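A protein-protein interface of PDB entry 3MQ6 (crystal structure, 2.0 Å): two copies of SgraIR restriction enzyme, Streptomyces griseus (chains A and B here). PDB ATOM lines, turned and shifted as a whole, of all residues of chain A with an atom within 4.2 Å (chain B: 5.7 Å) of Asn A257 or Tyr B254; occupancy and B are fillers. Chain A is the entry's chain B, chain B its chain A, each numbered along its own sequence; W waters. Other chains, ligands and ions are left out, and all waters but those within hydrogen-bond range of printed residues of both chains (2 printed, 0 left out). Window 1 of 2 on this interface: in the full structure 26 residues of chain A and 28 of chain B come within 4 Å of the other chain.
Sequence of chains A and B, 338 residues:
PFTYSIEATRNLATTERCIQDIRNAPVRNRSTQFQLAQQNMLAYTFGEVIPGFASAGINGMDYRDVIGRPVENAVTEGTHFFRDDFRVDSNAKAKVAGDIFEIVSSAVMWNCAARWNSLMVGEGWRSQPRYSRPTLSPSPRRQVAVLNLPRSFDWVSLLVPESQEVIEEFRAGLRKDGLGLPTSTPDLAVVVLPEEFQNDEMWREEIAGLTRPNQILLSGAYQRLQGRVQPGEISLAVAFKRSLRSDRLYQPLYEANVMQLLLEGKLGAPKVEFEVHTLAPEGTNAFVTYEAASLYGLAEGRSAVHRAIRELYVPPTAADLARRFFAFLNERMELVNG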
ATOM      1  N   TYR A 250      27.015  36.931  17.999  1.00  0.00           N
ATOM      2  CA  TYR A 250      26.971  35.522  18.405  1.00  0.00           C
ATOM      3  C   TYR A 250      25.641  34.774  18.478  1.00  0.00           C
ATOM      4  O   TYR A 250      25.633  33.548  18.419  1.00  0.00           O
ATOM      5  CB  TYR A 250      27.774  35.321  19.683  1.00  0.00           C
ATOM      6  CG  TYR A 250      29.232  35.549  19.421  1.00  0.00           C
ATOM      7  CD1 TYR A 250      30.002  34.584  18.767  1.00  0.00           C
ATOM      8  CD2 TYR A 250      29.832  36.737  19.770  1.00  0.00           C
ATOM      9  CE1 TYR A 250      31.343  34.794  18.509  1.00  0.00           C
ATOM     10  CE2 TYR A 250      31.192  36.969  19.504  1.00  0.00           C
ATOM     11  CZ  TYR A 250      31.939  35.992  18.876  1.00  0.00           C
ATOM     12  OH  TYR A 250      33.281  36.219  18.608  1.00  0.00           O
ATOM     13  N   LEU A 253      25.254  33.086  15.133  1.00  0.00           N
ATOM     14  CA  LEU A 253      26.295  32.082  14.946  1.00  0.00           C
ATOM     15  C   LEU A 253      25.927  30.846  15.753  1.00  0.00           C
ATOM     16  O   LEU A 253      25.991  29.708  15.279  1.00  0.00           O
ATOM     17  CB  LEU A 253      27.612  32.628  15.466  1.00  0.00           C
ATOM     18  CG  LEU A 253      28.825  31.739  15.235  1.00  0.00           C
ATOM     19  CD1 LEU A 253      28.878  31.353  13.777  1.00  0.00           C
ATOM     20  CD2 LEU A 253      30.064  32.494  15.635  1.00  0.00           C
ATOM     21  N   TYR A 254      25.538  31.079  16.999  1.00  0.00           N
ATOM     22  CA  TYR A 254      25.152  29.966  17.846  1.00  0.00           C
ATOM     23  C   TYR A 254      23.908  29.253  17.343  1.00  0.00           C
ATOM     24  O   TYR A 254      23.909  28.029  17.194  1.00  0.00           O
ATOM     25  CB  TYR A 254      24.965  30.377  19.298  1.00  0.00           C
ATOM     26  CG  TYR A 254      24.564  29.194  20.137  1.00  0.00           C
ATOM     27  CD1 TYR A 254      25.505  28.264  20.545  1.00  0.00           C
ATOM     28  CD2 TYR A 254      23.240  28.980  20.467  1.00  0.00           C
ATOM     29  CE1 TYR A 254      25.144  27.168  21.299  1.00  0.00           C
ATOM     30  CE2 TYR A 254      22.858  27.876  21.219  1.00  0.00           C
ATOM     31  CZ  TYR A 254      23.811  26.980  21.631  1.00  0.00           C
ATOM     32  OH  TYR A 254      23.442  25.880  22.370  1.00  0.00           O
ATOM     33  N   GLU A 255      22.853  30.014  17.071  1.00  0.00           N
ATOM     34  CA  GLU A 255      21.617  29.429  16.593  1.00  0.00           C
ATOM     35  C   GLU A 255      21.799  28.668  15.281  1.00  0.00           C
ATOM     36  O   GLU A 255      21.151  27.643  15.076  1.00  0.00           O
ATOM     37  CB  GLU A 255      20.526  30.490  16.430  1.00  0.00           C
ATOM     38  CG  GLU A 255      19.130  29.891  16.404  1.00  0.00           C
ATOM     39  CD  GLU A 255      18.786  29.150  17.692  1.00  0.00           C
ATOM     40  OE1 GLU A 255      19.340  29.503  18.761  1.00  0.00           O
ATOM     41  OE2 GLU A 255      17.949  28.225  17.642  1.00  0.00           O
ATOM     42  N   ALA A 256      22.668  29.158  14.392  1.00  0.00           N
ATOM     43  CA  ALA A 256      22.893  28.468  13.128  1.00  0.00           C
ATOM     44  C   ALA A 256      23.537  27.118  13.404  1.00  0.00           C
ATOM     45  O   ALA A 256      23.199  26.117  12.783  1.00  0.00           O
ATOM     46  CB  ALA A 256      23.761  29.296  12.170  1.00  0.00           C
ATOM     47  N   ASN A 257      24.471  27.106  14.344  1.00  0.00           N
ATOM     48  CA  ASN A 257      25.038  25.858  14.831  1.00  0.00           C
ATOM     49  C   ASN A 257      23.991  24.896  15.376  1.00  0.00           C
ATOM     50  O   ASN A 257      24.050  23.703  15.103  1.00  0.00           O
ATOM     51  CB  ASN A 257      26.111  26.135  15.874  1.00  0.00           C
ATOM     52  CG  ASN A 257      27.478  26.380  15.241  1.00  0.00           C
ATOM     53  OD1 ASN A 257      28.055  25.475  14.650  1.00  0.00           O
ATOM     54  ND2 ASN A 257      27.999  27.602  15.370  1.00  0.00           N
ATOM     55  N   VAL A 258      23.025  25.401  16.133  1.00  0.00           N
ATOM     56  CA  VAL A 258      22.013  24.512  16.688  1.00  0.00           C
ATOM     57  C   VAL A 258      21.095  24.005  15.577  1.00  0.00           C
ATOM     58  O   VAL A 258      20.785  22.815  15.526  1.00  0.00           O
ATOM     59  CB  VAL A 258      21.242  25.153  17.857  1.00  0.00           C
ATOM     60  CG1 VAL A 258      20.090  24.255  18.313  1.00  0.00           C
ATOM     61  CG2 VAL A 258      22.196  25.408  19.012  1.00  0.00           C
ATOM     62  N   MET A 259      20.705  24.894  14.667  1.00  0.00           N
ATOM     63  CA  MET A 259      19.882  24.508  13.528  1.00  0.00           C
ATOM     64  C   MET A 259      20.571  23.384  12.740  1.00  0.00           C
ATOM     65  O   MET A 259      19.927  22.446  12.279  1.00  0.00           O
ATOM     66  CB  MET A 259      19.571  25.713  12.612  1.00  0.00           C
ATOM     67  CG  MET A 259      18.836  26.871  13.277  1.00  0.00           C
ATOM     68  SD  MET A 259      18.145  28.098  12.134  1.00  0.00           S
ATOM     69  CE  MET A 259      17.210  27.087  11.012  1.00  0.00           C
ATOM     70  N   GLN A 260      21.887  23.456  12.616  1.00  0.00           N
ATOM     71  CA  GLN A 260      22.591  22.473  11.807  1.00  0.00           C
ATOM     72  C   GLN A 260      22.757  21.149  12.541  1.00  0.00           C
ATOM     73  O   GLN A 260      22.622  20.083  11.936  1.00  0.00           O
ATOM     74  CB  GLN A 260      23.917  23.039  11.305  1.00  0.00           C
ATOM     75  CG  GLN A 260      23.691  24.172  10.326  1.00  0.00           C
ATOM     76  CD  GLN A 260      24.914  25.040  10.128  1.00  0.00           C
ATOM     77  OE1 GLN A 260      25.926  24.866  10.809  1.00  0.00           O
ATOM     78  NE2 GLN A 260      24.830  25.988   9.187  1.00  0.00           N
ATOM     79  N   LEU A 261      22.998  21.208  13.848  1.00  0.00           N
ATOM     80  CA  LEU A 261      23.065  19.982  14.629  1.00  0.00           C
ATOM     81  C   LEU A 261      21.762  19.209  14.498  1.00  0.00           C
ATOM     82  O   LEU A 261      21.773  18.031  14.129  1.00  0.00           O
ATOM     83  CB  LEU A 261      23.404  20.242  16.099  1.00  0.00           C
ATOM     84  CG  LEU A 261      23.609  18.949  16.894  1.00  0.00           C
ATOM     85  CD1 LEU A 261      24.528  19.168  18.076  1.00  0.00           C
ATOM     86  CD2 LEU A 261      22.275  18.364  17.337  1.00  0.00           C
ATOM     87  N   ALA A 292      33.614  30.900  10.606  1.00  0.00           N
ATOM     88  CA  ALA A 292      33.589  29.791  11.536  1.00  0.00           C
ATOM     89  C   ALA A 292      32.909  28.577  10.915  1.00  0.00           C
ATOM     90  O   ALA A 292      31.848  28.691  10.298  1.00  0.00           O
ATOM     91  CB  ALA A 292      32.882  30.200  12.822  1.00  0.00           C
ATOM     92  N   SER A 294      30.833  25.052  11.003  1.00  0.00           N
ATOM     93  CA  SER A 294      29.759  24.474  11.802  1.00  0.00           C
ATOM     94  C   SER A 294      30.332  23.471  12.800  1.00  0.00           C
ATOM     95  O   SER A 294      30.961  22.489  12.402  1.00  0.00           O
ATOM     96  CB  SER A 294      28.736  23.789  10.895  1.00  0.00           C
ATOM     97  OG  SER A 294      27.854  22.980  11.650  1.00  0.00           O
ATOM     98  N   LEU A 295      30.106  23.718  14.090  1.00  0.00           N
ATOM     99  CA  LEU A 295      30.707  22.916  15.154  1.00  0.00           C
ATOM    100  C   LEU A 295      30.315  21.441  15.057  1.00  0.00           C
ATOM    101  O   LEU A 295      31.151  20.557  15.220  1.00  0.00           O
ATOM    102  CB  LEU A 295      30.329  23.476  16.530  1.00  0.00           C
ATOM    103  CG  LEU A 295      30.866  24.877  16.834  1.00  0.00           C
ATOM    104  CD1 LEU A 295      30.740  25.194  18.306  1.00  0.00           C
ATOM    105  CD2 LEU A 295      32.324  25.018  16.399  1.00  0.00           C
ATOM    106  N   ALA A 308      29.134  27.908   9.438  1.00  0.00           N
ATOM    107  CA  ALA A 308      27.845  28.022  10.105  1.00  0.00           C
ATOM    108  C   ALA A 308      27.042  29.118   9.425  1.00  0.00           C
ATOM    109  O   ALA A 308      25.867  28.930   9.084  1.00  0.00           O
ATOM    110  CB  ALA A 308      28.023  28.304  11.593  1.00  0.00           C
ATOM    111  N   LEU B 181      38.278  28.581  12.548  1.00  0.00           N
ATOM    112  CA  LEU B 181      37.613  28.468  13.834  1.00  0.00           C
ATOM    113  C   LEU B 181      38.253  29.456  14.796  1.00  0.00           C
ATOM    114  O   LEU B 181      38.951  29.070  15.725  1.00  0.00           O
ATOM    115  CB  LEU B 181      37.652  27.036  14.384  1.00  0.00           C
ATOM    116  CG  LEU B 181      36.730  26.769  15.590  1.00  0.00           C
ATOM    117  CD1 LEU B 181      35.258  27.093  15.258  1.00  0.00           C
ATOM    118  CD2 LEU B 181      36.860  25.342  16.090  1.00  0.00           C
ATOM    119  N   PRO B 182      37.996  30.748  14.574  1.00  0.00           N
ATOM    120  CA  PRO B 182      38.556  31.805  15.417  1.00  0.00           C
ATOM    121  C   PRO B 182      38.185  31.568  16.872  1.00  0.00           C
ATOM    122  O   PRO B 182      37.079  31.091  17.152  1.00  0.00           O
ATOM    123  CB  PRO B 182      37.851  33.071  14.910  1.00  0.00           C
ATOM    124  CG  PRO B 182      37.283  32.709  13.577  1.00  0.00           C
ATOM    125  CD  PRO B 182      36.971  31.256  13.648  1.00  0.00           C
ATOM    126  N   TYR B 250      24.866  35.090  24.125  1.00  0.00           N
ATOM    127  CA  TYR B 250      25.464  34.034  23.288  1.00  0.00           C
ATOM    128  C   TYR B 250      26.966  33.986  23.111  1.00  0.00           C
ATOM    129  O   TYR B 250      27.513  32.935  22.764  1.00  0.00           O
ATOM    130  CB  TYR B 250      24.732  33.993  21.935  1.00  0.00           C
ATOM    131  CG  TYR B 250      23.320  33.539  22.164  1.00  0.00           C
ATOM    132  CD1 TYR B 250      23.038  32.189  22.317  1.00  0.00           C
ATOM    133  CD2 TYR B 250      22.281  34.458  22.309  1.00  0.00           C
ATOM    134  CE1 TYR B 250      21.759  31.756  22.559  1.00  0.00           C
ATOM    135  CE2 TYR B 250      20.992  34.035  22.545  1.00  0.00           C
ATOM    136  CZ  TYR B 250      20.739  32.671  22.678  1.00  0.00           C
ATOM    137  OH  TYR B 250      19.467  32.215  22.926  1.00  0.00           O
ATOM    138  N   GLN B 251      27.648  35.103  23.334  1.00  0.00           N
ATOM    139  CA  GLN B 251      29.096  35.112  23.176  1.00  0.00           C
ATOM    140  C   GLN B 251      29.739  34.133  24.146  1.00  0.00           C
ATOM    141  O   GLN B 251      30.607  33.347  23.760  1.00  0.00           O
ATOM    142  CB  GLN B 251      29.685  36.539  23.323  1.00  0.00           C
ATOM    143  CG  GLN B 251      31.221  36.609  23.188  1.00  0.00           C
ATOM    144  CD  GLN B 251      31.936  36.193  24.461  1.00  0.00           C
ATOM    145  OE1 GLN B 251      31.407  36.354  25.565  1.00  0.00           O
ATOM    146  NE2 GLN B 251      33.136  35.647  24.316  1.00  0.00           N
ATOM    147  N   PRO B 252      29.300  34.140  25.414  1.00  0.00           N
ATOM    148  CA  PRO B 252      29.917  33.177  26.326  1.00  0.00           C
ATOM    149  C   PRO B 252      29.494  31.750  26.011  1.00  0.00           C
ATOM    150  O   PRO B 252      30.309  30.843  26.137  1.00  0.00           O
ATOM    151  CB  PRO B 252      29.361  33.574  27.699  1.00  0.00           C
ATOM    152  CG  PRO B 252      28.870  34.943  27.539  1.00  0.00           C
ATOM    153  CD  PRO B 252      28.405  35.067  26.122  1.00  0.00           C
ATOM    154  N   LEU B 253      28.239  31.547  25.624  1.00  0.00           N
ATOM    155  CA  LEU B 253      27.789  30.198  25.272  1.00  0.00           C
ATOM    156  C   LEU B 253      28.561  29.648  24.068  1.00  0.00           C
ATOM    157  O   LEU B 253      29.087  28.526  24.095  1.00  0.00           O
ATOM    158  CB  LEU B 253      26.297  30.188  24.971  1.00  0.00           C
ATOM    159  CG  LEU B 253      25.736  28.801  24.657  1.00  0.00           C
ATOM    160  CD1 LEU B 253      26.029  27.831  25.795  1.00  0.00           C
ATOM    161  CD2 LEU B 253      24.239  28.918  24.422  1.00  0.00           C
ATOM    162  N   TYR B 254      28.629  30.445  23.010  1.00  0.00           N
ATOM    163  CA  TYR B 254      29.439  30.085  21.844  1.00  0.00           C
ATOM    164  C   TYR B 254      30.919  29.838  22.177  1.00  0.00           C
ATOM    165  O   TYR B 254      31.547  28.886  21.705  1.00  0.00           O
ATOM    166  CB  TYR B 254      29.322  31.121  20.713  1.00  0.00           C
ATOM    167  CG  TYR B 254      30.116  30.646  19.506  1.00  0.00           C
ATOM    168  CD1 TYR B 254      29.591  29.681  18.647  1.00  0.00           C
ATOM    169  CD2 TYR B 254      31.414  31.072  19.285  1.00  0.00           C
ATOM    170  CE1 TYR B 254      30.322  29.197  17.568  1.00  0.00           C
ATOM    171  CE2 TYR B 254      32.160  30.589  18.198  1.00  0.00           C
ATOM    172  CZ  TYR B 254      31.602  29.644  17.351  1.00  0.00           C
ATOM    173  OH  TYR B 254      32.324  29.128  16.288  1.00  0.00           O
ATOM    174  N   GLU B 255      31.512  30.713  22.968  1.00  0.00           N
ATOM    175  CA  GLU B 255      32.937  30.600  23.160  1.00  0.00           C
ATOM    176  C   GLU B 255      33.269  29.379  24.016  1.00  0.00           C
ATOM    177  O   GLU B 255      34.295  28.731  23.812  1.00  0.00           O
ATOM    178  CB  GLU B 255      33.517  31.879  23.770  1.00  0.00           C
ATOM    179  CG  GLU B 255      35.044  31.915  23.722  1.00  0.00           C
ATOM    180  CD  GLU B 255      35.583  32.052  22.305  1.00  0.00           C
ATOM    181  OE1 GLU B 255      36.756  31.672  22.065  1.00  0.00           O
ATOM    182  OE2 GLU B 255      34.826  32.534  21.428  1.00  0.00           O
ATOM    183  N   ALA B 256      32.380  29.053  24.954  1.00  0.00           N
ATOM    184  CA  ALA B 256      32.563  27.896  25.822  1.00  0.00           C
ATOM    185  C   ALA B 256      32.504  26.633  24.966  1.00  0.00           C
ATOM    186  O   ALA B 256      33.289  25.697  25.149  1.00  0.00           O
ATOM    187  CB  ALA B 256      31.482  27.867  26.895  1.00  0.00           C
ATOM    188  N   ASN B 257      31.578  26.632  24.012  1.00  0.00           N
ATOM    189  CA  ASN B 257      31.492  25.548  23.046  1.00  0.00           C
ATOM    190  C   ASN B 257      32.791  25.394  22.278  1.00  0.00           C
ATOM    191  O   ASN B 257      33.295  24.284  22.145  1.00  0.00           O
ATOM    192  CB  ASN B 257      30.332  25.761  22.084  1.00  0.00           C
ATOM    193  CG  ASN B 257      29.049  25.149  22.586  1.00  0.00           C
ATOM    194  OD1 ASN B 257      28.891  23.934  22.587  1.00  0.00           O
ATOM    195  ND2 ASN B 257      28.100  25.998  22.984  1.00  0.00           N
ATOM    196  N   VAL B 258      33.343  26.508  21.787  1.00  0.00           N
ATOM    197  CA  VAL B 258      34.612  26.462  21.060  1.00  0.00           C
ATOM    198  C   VAL B 258      35.774  26.010  21.958  1.00  0.00           C
ATOM    199  O   VAL B 258      36.595  25.191  21.545  1.00  0.00           O
ATOM    200  CB  VAL B 258      34.943  27.801  20.364  1.00  0.00           C
ATOM    201  CG1 VAL B 258      36.372  27.786  19.824  1.00  0.00           C
ATOM    202  CG2 VAL B 258      33.960  28.057  19.238  1.00  0.00           C
ATOM    203  N   MET B 259      35.836  26.532  23.178  1.00  0.00           N
ATOM    204  CA  MET B 259      36.833  26.091  24.157  1.00  0.00           C
ATOM    205  C   MET B 259      36.738  24.607  24.484  1.00  0.00           C
ATOM    206  O   MET B 259      37.757  23.941  24.664  1.00  0.00           O
ATOM    207  CB  MET B 259      36.727  26.887  25.459  1.00  0.00           C
ATOM    208  CG  MET B 259      37.260  28.322  25.379  1.00  0.00           C
ATOM    209  SD  MET B 259      37.183  29.156  26.994  1.00  0.00           S
ATOM    210  CE  MET B 259      37.962  27.955  28.069  1.00  0.00           C
ATOM    211  N   LEU B 295      27.932  21.253  22.410  1.00  0.00           N
ATOM    212  CA  LEU B 295      27.638  20.726  21.079  1.00  0.00           C
ATOM    213  C   LEU B 295      28.681  19.726  20.607  1.00  0.00           C
ATOM    214  O   LEU B 295      28.348  18.741  19.947  1.00  0.00           O
ATOM    215  CB  LEU B 295      27.559  21.855  20.049  1.00  0.00           C
ATOM    216  CG  LEU B 295      26.524  22.956  20.235  1.00  0.00           C
ATOM    217  CD1 LEU B 295      26.421  23.763  18.955  1.00  0.00           C
ATOM    218  CD2 LEU B 295      25.191  22.366  20.609  1.00  0.00           C
HETATM  219  O   HOH W   1      25.681  24.714  24.015  1.00  0.00           O
HETATM  220  O   HOH W   2      30.647  27.716  14.350  1.00  0.00           O
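Asn A257 touches just these residues of chain B: Tyr B254 and Leu B295.
Printed residues of chain B within 4 Å of Ala A292: Tyr B254 (3.7 Å).
Of chain A, only Tyr A250 (3.8 Å), Leu A253 (3.7 Å), Asn A257 (3.6 Å) and Ala A292 (3.7 Å) come within 4 Å of Tyr B254.
Glu B255 touches none of the printed residues of chain A.
Printed residues of chain A within 4 Å of Asn B257: Tyr A254 and Leu A295.
Met B259 touches none of the printed residues of chain A.
The nearest residue of chain A that does not touch Tyr B254 is Leu A295 (4.1 Å).
Of the 13 printed residues of chain B, 7 touch a printed residue of chain A.
Hydrophobic or aromatic side chains of chain A that line the printed part of chain B: Tyr A250, Leu A253, Tyr A254, Ala A292 and Leu A295.
Tyr B250 touches its own counterpart, Tyr A250.
Tyr A250 touches Tyr B254, and with the chains exchanged Tyr A254 touches Tyr B250.
Tyr A254 touches Asn B257, and with the chains exchanged Asn A257 touches Tyr B254.
Asn A257 touches Leu B295, and with the chains exchanged Leu A295 touches Asn B257.
Positions printed for both chains: 250, 253, 254, 255, 256, 257, 258, 259 and 295.
Of the 12 pairs that touch across the chains among the printed residues, 9 have their exchanged pair printed and touching as well.
Water W2 bridges ND2 of Asn A257 (2.8 Å) and OH of Tyr B254 (2.9 Å).
Water W1 lies within hydrogen-bond range of ND2 of Asn B257 and OH of Tyr A254.
O of Leu B253 lies within hydrogen-bond range of ND2 of Asn B257 (2.9 Å).
OD1 of Asn A257 is in hydrogen-bond range of N of Leu A295, at 2.8 Å.
O of Leu A253 lies within hydrogen-bond range of ND2 of Asn A257 (2.9 Å).
N of Ala A308 lies within hydrogen-bond range of O of Ala A292 (3.0 Å).
The side-chain amide oxygen (OD1) of Asn B257 is in hydrogen-bond range of the backbone NH (N) of Leu B295, at 2.9 Å.
Among the printed residues, merely in contact across the chains: Tyr A250 with Tyr B250 (3.7 Å), Tyr A250 with Gln B251 (3.6 Å), Tyr A250 with Tyr B254 (3.8 Å), Leu A253 with Tyr B254 (3.7 Å), Tyr A254 with Tyr B250 (3.7 Å), Tyr A254 with Leu B253 (3.4 Å), Tyr A254 with Asn B257 (3.6 Å), Asn A257 with Tyr B254 (3.6 Å), Asn A257 with Leu B295 (3.9 Å), Ala A292 with Tyr B254 (3.7 Å), Leu A295 with Leu B181 (3.8 Å) and Leu A295 with Asn B257 (3.8 Å).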
